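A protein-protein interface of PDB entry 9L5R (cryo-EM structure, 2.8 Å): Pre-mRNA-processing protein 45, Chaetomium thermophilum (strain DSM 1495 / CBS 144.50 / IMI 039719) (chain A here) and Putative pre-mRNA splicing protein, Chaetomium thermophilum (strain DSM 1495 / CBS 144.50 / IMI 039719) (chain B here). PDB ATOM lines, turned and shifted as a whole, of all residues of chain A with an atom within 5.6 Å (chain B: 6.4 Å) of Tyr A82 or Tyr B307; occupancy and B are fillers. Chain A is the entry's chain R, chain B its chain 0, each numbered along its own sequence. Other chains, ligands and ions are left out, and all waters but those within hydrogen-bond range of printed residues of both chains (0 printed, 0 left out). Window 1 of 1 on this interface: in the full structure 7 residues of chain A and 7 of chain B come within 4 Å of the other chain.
Tyr A82 touches just one residue of chain B: Tyr B307. Trp A84 touches none of the printed residues of chain B. Printed residues of chain B within 4 Å of Lys A86: Glu B308. Tyr B307 touches just one residue of chain A: Tyr A82. Of the printed residues of chain A, Glu B308 touches Lys A86 (3.3 Å). The nearest residue of chain B that does not touch Tyr A82 is Gly B306 (4.2 Å).
OH of Tyr A82 lies within hydrogen-bond range of NZ of Lys A86 (2.9 Å).
The side-chain amino group (NZ) of Lys A86 lies within salt-bridge range of the side-chain carboxylate (OE2) of Glu B308 (3.3 Å).
Ala A80 touches Leu B304 (N to CD2, 3.8 Å). Glu B305 touches Ala A80 (O to N, 3.98 Å). CB of Ala A80 touches O of Gly B306, 3.7 Å away. Tyr A82 touches Tyr B307 (OH to O, 3.9 Å).
Of the 11 printed residues of chain B, 5 touch a printed residue of chain A. Hydrophobic or aromatic side chains of chain A that line the printed part of chain B: Ala A80 and Tyr A82. Among the printed residues, 5 pairs touch across the chains.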
ATOM      1  N   ALA A  64     -34.634   1.208  10.111  1.00  0.00           N
ATOM      2  CA  ALA A  64     -34.421   2.641   9.988  1.00  0.00           C
ATOM      3  C   ALA A  64     -34.387   3.256  11.382  1.00  0.00           C
ATOM      4  O   ALA A  64     -34.850   2.638  12.356  1.00  0.00           O
ATOM      5  CB  ALA A  64     -35.523   3.290   9.134  1.00  0.00           C
ATOM      6  N   PRO A  65     -33.852   4.476  11.513  1.00  0.00           N
ATOM      7  CA  PRO A  65     -33.967   5.191  12.792  1.00  0.00           C
ATOM      8  C   PRO A  65     -35.400   5.460  13.233  1.00  0.00           C
ATOM      9  O   PRO A  65     -35.612   5.730  14.424  1.00  0.00           O
ATOM     10  CB  PRO A  65     -33.197   6.488  12.528  1.00  0.00           C
ATOM     11  CG  PRO A  65     -32.178   6.101  11.523  1.00  0.00           C
ATOM     12  CD  PRO A  65     -32.833   5.087  10.639  1.00  0.00           C
ATOM     13  N   PHE A  68     -35.604   2.471  15.290  1.00  0.00           N
ATOM     14  CA  PHE A  68     -34.890   2.681  16.545  1.00  0.00           C
ATOM     15  C   PHE A  68     -35.618   3.645  17.472  1.00  0.00           C
ATOM     16  O   PHE A  68     -35.392   3.608  18.685  1.00  0.00           O
ATOM     17  CB  PHE A  68     -33.472   3.172  16.271  1.00  0.00           C
ATOM     18  CG  PHE A  68     -32.648   2.189  15.516  1.00  0.00           C
ATOM     19  CD1 PHE A  68     -32.187   1.048  16.130  1.00  0.00           C
ATOM     20  CD2 PHE A  68     -32.361   2.389  14.186  1.00  0.00           C
ATOM     21  CE1 PHE A  68     -31.450   0.139  15.434  1.00  0.00           C
ATOM     22  CE2 PHE A  68     -31.624   1.481  13.481  1.00  0.00           C
ATOM     23  CZ  PHE A  68     -31.170   0.356  14.102  1.00  0.00           C
ATOM     24  N   ALA A  80     -25.841  -5.878  12.588  1.00  0.00           N
ATOM     25  CA  ALA A  80     -25.285  -4.562  12.870  1.00  0.00           C
ATOM     26  C   ALA A  80     -26.353  -3.489  12.710  1.00  0.00           C
ATOM     27  O   ALA A  80     -27.048  -3.443  11.692  1.00  0.00           O
ATOM     28  CB  ALA A  80     -24.111  -4.275  11.938  1.00  0.00           C
ATOM     29  N   GLN A  81     -26.477  -2.619  13.707  1.00  0.00           N
ATOM     30  CA  GLN A  81     -27.470  -1.558  13.686  1.00  0.00           C
ATOM     31  C   GLN A  81     -26.812  -0.185  13.666  1.00  0.00           C
ATOM     32  O   GLN A  81     -25.705   0.002  14.175  1.00  0.00           O
ATOM     33  CB  GLN A  81     -28.430  -1.617  14.882  1.00  0.00           C
ATOM     34  CG  GLN A  81     -29.463  -2.732  14.846  1.00  0.00           C
ATOM     35  CD  GLN A  81     -29.032  -3.953  15.590  1.00  0.00           C
ATOM     36  OE1 GLN A  81     -28.171  -3.881  16.451  1.00  0.00           O
ATOM     37  NE2 GLN A  81     -29.608  -5.092  15.251  1.00  0.00           N
ATOM     38  N   TYR A  82     -27.520   0.777  13.078  1.00  0.00           N
ATOM     39  CA  TYR A  82     -27.069   2.160  12.958  1.00  0.00           C
ATOM     40  C   TYR A  82     -28.214   3.072  13.369  1.00  0.00           C
ATOM     41  O   TYR A  82     -29.058   3.431  12.538  1.00  0.00           O
ATOM     42  CB  TYR A  82     -26.611   2.472  11.537  1.00  0.00           C
ATOM     43  CG  TYR A  82     -25.596   1.503  10.992  1.00  0.00           C
ATOM     44  CD1 TYR A  82     -24.243   1.713  11.184  1.00  0.00           C
ATOM     45  CD2 TYR A  82     -25.988   0.381  10.285  1.00  0.00           C
ATOM     46  CE1 TYR A  82     -23.309   0.833  10.691  1.00  0.00           C
ATOM     47  CE2 TYR A  82     -25.063  -0.505   9.793  1.00  0.00           C
ATOM     48  CZ  TYR A  82     -23.726  -0.273   9.997  1.00  0.00           C
ATOM     49  OH  TYR A  82     -22.798  -1.154   9.500  1.00  0.00           O
ATOM     50  N   PRO A  83     -28.287   3.451  14.646  1.00  0.00           N
ATOM     51  CA  PRO A  83     -29.404   4.289  15.112  1.00  0.00           C
ATOM     52  C   PRO A  83     -29.476   5.670  14.478  1.00  0.00           C
ATOM     53  O   PRO A  83     -30.542   6.290  14.514  1.00  0.00           O
ATOM     54  CB  PRO A  83     -29.155   4.387  16.621  1.00  0.00           C
ATOM     55  CG  PRO A  83     -28.372   3.188  16.946  1.00  0.00           C
ATOM     56  CD  PRO A  83     -27.495   2.930  15.767  1.00  0.00           C
ATOM     57  N   TRP A  84     -28.386   6.184  13.914  1.00  0.00           N
ATOM     58  CA  TRP A  84     -28.416   7.480  13.249  1.00  0.00           C
ATOM     59  C   TRP A  84     -27.860   7.415  11.832  1.00  0.00           C
ATOM     60  O   TRP A  84     -27.478   8.444  11.274  1.00  0.00           O
ATOM     61  CB  TRP A  84     -27.668   8.532  14.069  1.00  0.00           C
ATOM     62  CG  TRP A  84     -26.234   8.220  14.401  1.00  0.00           C
ATOM     63  CD1 TRP A  84     -25.207   8.034  13.529  1.00  0.00           C
ATOM     64  CD2 TRP A  84     -25.669   8.111  15.709  1.00  0.00           C
ATOM     65  NE1 TRP A  84     -24.045   7.795  14.209  1.00  0.00           N
ATOM     66  CE2 TRP A  84     -24.303   7.839  15.553  1.00  0.00           C
ATOM     67  CE3 TRP A  84     -26.191   8.210  16.997  1.00  0.00           C
ATOM     68  CZ2 TRP A  84     -23.453   7.663  16.635  1.00  0.00           C
ATOM     69  CZ3 TRP A  84     -25.349   8.034  18.067  1.00  0.00           C
ATOM     70  CH2 TRP A  84     -23.999   7.765  17.883  1.00  0.00           C
ATOM     71  N   GLY A  85     -27.795   6.234  11.247  1.00  0.00           N
ATOM     72  CA  GLY A  85     -27.371   6.145   9.869  1.00  0.00           C
ATOM     73  C   GLY A  85     -25.979   5.569   9.722  1.00  0.00           C
ATOM     74  O   GLY A  85     -25.103   5.747  10.575  1.00  0.00           O
ATOM     75  N   LYS A  86     -25.775   4.852   8.623  1.00  0.00           N
ATOM     76  CA  LYS A  86     -24.466   4.311   8.288  1.00  0.00           C
ATOM     77  C   LYS A  86     -23.506   5.434   7.931  1.00  0.00           C
ATOM     78  O   LYS A  86     -23.897   6.439   7.331  1.00  0.00           O
ATOM     79  CB  LYS A  86     -24.587   3.345   7.108  1.00  0.00           C
ATOM     80  CG  LYS A  86     -23.313   2.602   6.739  1.00  0.00           C
ATOM     81  CD  LYS A  86     -23.545   1.676   5.558  1.00  0.00           C
ATOM     82  CE  LYS A  86     -24.394   0.477   5.924  1.00  0.00           C
ATOM     83  NZ  LYS A  86     -23.674  -0.420   6.863  1.00  0.00           N
ATOM     84  N   ASN A  87     -22.246   5.271   8.318  1.00  0.00           N
ATOM     85  CA  ASN A  87     -21.160   6.070   7.763  1.00  0.00           C
ATOM     86  C   ASN A  87     -20.567   5.293   6.596  1.00  0.00           C
ATOM     87  O   ASN A  87     -20.078   4.172   6.773  1.00  0.00           O
ATOM     88  CB  ASN A  87     -20.098   6.378   8.815  1.00  0.00           C
ATOM     89  CG  ASN A  87     -20.427   7.608   9.623  1.00  0.00           C
ATOM     90  OD1 ASN A  87     -20.824   8.631   9.072  1.00  0.00           O
ATOM     91  ND2 ASN A  87     -20.256   7.520  10.935  1.00  0.00           N
ATOM     92  N   SER B 300     -13.412  -9.239   8.552  1.00  0.00           N
ATOM     93  CA  SER B 300     -13.988  -7.924   8.783  1.00  0.00           C
ATOM     94  C   SER B 300     -15.368  -8.009   9.411  1.00  0.00           C
ATOM     95  O   SER B 300     -15.822  -7.032  10.013  1.00  0.00           O
ATOM     96  CB  SER B 300     -14.052  -7.150   7.470  1.00  0.00           C
ATOM     97  OG  SER B 300     -14.827  -5.978   7.615  1.00  0.00           O
ATOM     98  N   SER B 301     -16.051  -9.147   9.278  1.00  0.00           N
ATOM     99  CA  SER B 301     -17.338  -9.307   9.939  1.00  0.00           C
ATOM    100  C   SER B 301     -17.170  -9.454  11.441  1.00  0.00           C
ATOM    101  O   SER B 301     -17.908  -8.821  12.206  1.00  0.00           O
ATOM    102  CB  SER B 301     -18.088 -10.507   9.362  1.00  0.00           C
ATOM    103  OG  SER B 301     -18.055 -10.501   7.947  1.00  0.00           O
ATOM    104  N   TYR B 302     -16.202 -10.275  11.877  1.00  0.00           N
ATOM    105  CA  TYR B 302     -15.927 -10.502  13.308  1.00  0.00           C
ATOM    106  C   TYR B 302     -17.163 -11.008  14.053  1.00  0.00           C
ATOM    107  O   TYR B 302     -17.537 -10.474  15.097  1.00  0.00           O
ATOM    108  CB  TYR B 302     -15.402  -9.239  14.009  1.00  0.00           C
ATOM    109  CG  TYR B 302     -13.965  -8.857  13.766  1.00  0.00           C
ATOM    110  CD1 TYR B 302     -12.927  -9.689  14.157  1.00  0.00           C
ATOM    111  CD2 TYR B 302     -13.645  -7.630  13.202  1.00  0.00           C
ATOM    112  CE1 TYR B 302     -11.611  -9.328  13.950  1.00  0.00           C
ATOM    113  CE2 TYR B 302     -12.335  -7.261  12.992  1.00  0.00           C
ATOM    114  CZ  TYR B 302     -11.324  -8.113  13.368  1.00  0.00           C
ATOM    115  OH  TYR B 302     -10.016  -7.749  13.160  1.00  0.00           O
ATOM    116  N   LEU B 304     -20.819 -10.787  13.733  1.00  0.00           N
ATOM    117  CA  LEU B 304     -22.007 -10.172  13.130  1.00  0.00           C
ATOM    118  C   LEU B 304     -22.017 -10.203  11.609  1.00  0.00           C
ATOM    119  O   LEU B 304     -20.994  -9.996  10.952  1.00  0.00           O
ATOM    120  CB  LEU B 304     -22.149  -8.716  13.582  1.00  0.00           C
ATOM    121  CG  LEU B 304     -22.812  -8.334  14.900  1.00  0.00           C
ATOM    122  CD1 LEU B 304     -22.020  -8.732  16.107  1.00  0.00           C
ATOM    123  CD2 LEU B 304     -22.988  -6.835  14.872  1.00  0.00           C
ATOM    124  N   GLU B 305     -23.200 -10.466  11.067  1.00  0.00           N
ATOM    125  CA  GLU B 305     -23.417 -10.457   9.633  1.00  0.00           C
ATOM    126  C   GLU B 305     -23.608  -9.028   9.143  1.00  0.00           C
ATOM    127  O   GLU B 305     -24.320  -8.233   9.764  1.00  0.00           O
ATOM    128  CB  GLU B 305     -24.643 -11.300   9.287  1.00  0.00           C
ATOM    129  CG  GLU B 305     -25.791 -11.120  10.269  1.00  0.00           C
ATOM    130  CD  GLU B 305     -26.946 -12.059  10.000  1.00  0.00           C
ATOM    131  OE1 GLU B 305     -26.818 -12.918   9.105  1.00  0.00           O
ATOM    132  OE2 GLU B 305     -27.984 -11.935  10.683  1.00  0.00           O
ATOM    133  N   GLY B 306     -22.974  -8.710   8.018  1.00  0.00           N
ATOM    134  CA  GLY B 306     -23.085  -7.385   7.444  1.00  0.00           C
ATOM    135  C   GLY B 306     -22.495  -6.285   8.298  1.00  0.00           C
ATOM    136  O   GLY B 306     -23.142  -5.257   8.519  1.00  0.00           O
ATOM    137  N   TYR B 307     -21.277  -6.486   8.805  1.00  0.00           N
ATOM    138  CA  TYR B 307     -20.623  -5.426   9.562  1.00  0.00           C
ATOM    139  C   TYR B 307     -19.672  -4.609   8.691  1.00  0.00           C
ATOM    140  O   TYR B 307     -19.750  -3.375   8.699  1.00  0.00           O
ATOM    141  CB  TYR B 307     -19.879  -6.001  10.769  1.00  0.00           C
ATOM    142  CG  TYR B 307     -19.085  -4.951  11.513  1.00  0.00           C
ATOM    143  CD1 TYR B 307     -19.653  -3.726  11.844  1.00  0.00           C
ATOM    144  CD2 TYR B 307     -17.768  -5.175  11.871  1.00  0.00           C
ATOM    145  CE1 TYR B 307     -18.930  -2.763  12.495  1.00  0.00           C
ATOM    146  CE2 TYR B 307     -17.043  -4.216  12.540  1.00  0.00           C
ATOM    147  CZ  TYR B 307     -17.631  -3.014  12.847  1.00  0.00           C
ATOM    148  OH  TYR B 307     -16.916  -2.048  13.511  1.00  0.00           O
ATOM    149  N   GLU B 308     -18.819  -5.279   7.911  1.00  0.00           N
ATOM    150  CA  GLU B 308     -17.794  -4.665   7.054  1.00  0.00           C
ATOM    151  C   GLU B 308     -17.003  -3.574   7.798  1.00  0.00           C
ATOM    152  O   GLU B 308     -17.142  -2.374   7.566  1.00  0.00           O
ATOM    153  CB  GLU B 308     -18.346  -4.201   5.682  1.00  0.00           C
ATOM    154  CG  GLU B 308     -19.349  -3.016   5.519  1.00  0.00           C
ATOM    155  CD  GLU B 308     -20.826  -3.373   5.666  1.00  0.00           C
ATOM    156  OE1 GLU B 308     -21.169  -4.456   6.169  1.00  0.00           O
ATOM    157  OE2 GLU B 308     -21.663  -2.535   5.272  1.00  0.00           O
ATOM    158  N   ALA B 309     -16.196  -4.050   8.764  1.00  0.00           N
ATOM    159  CA  ALA B 309     -15.291  -3.266   9.609  1.00  0.00           C
ATOM    160  C   ALA B 309     -14.501  -2.213   8.843  1.00  0.00           C
ATOM    161  O   ALA B 309     -14.166  -2.423   7.671  1.00  0.00           O
ATOM    162  CB  ALA B 309     -14.303  -4.182  10.331  1.00  0.00           C
ATOM    163  N   PRO B 310     -14.210  -1.069   9.463  1.00  0.00           N
ATOM    164  CA  PRO B 310     -13.388  -0.054   8.797  1.00  0.00           C
ATOM    165  C   PRO B 310     -11.993  -0.577   8.502  1.00  0.00           C
ATOM    166  O   PRO B 310     -11.476  -1.454   9.195  1.00  0.00           O
ATOM    167  CB  PRO B 310     -13.345   1.090   9.815  1.00  0.00           C
ATOM    168  CG  PRO B 310     -14.556   0.896  10.648  1.00  0.00           C
ATOM    169  CD  PRO B 310     -14.756  -0.579  10.739  1.00  0.00           C
ATOM    170  N   VAL B 313      -9.633   0.073  11.442  1.00  0.00           N
ATOM    171  CA  VAL B 313      -9.753  -0.874  12.546  1.00  0.00           C
ATOM    172  C   VAL B 313      -9.205  -2.234  12.144  1.00  0.00           C
ATOM    173  O   VAL B 313      -8.537  -2.909  12.935  1.00  0.00           O
ATOM    174  CB  VAL B 313     -11.216  -0.982  13.012  1.00  0.00           C
ATOM    175  CG1 VAL B 313     -11.305  -1.820  14.272  1.00  0.00           C
ATOM    176  CG2 VAL B 313     -11.820   0.379  13.226  1.00  0.00           C
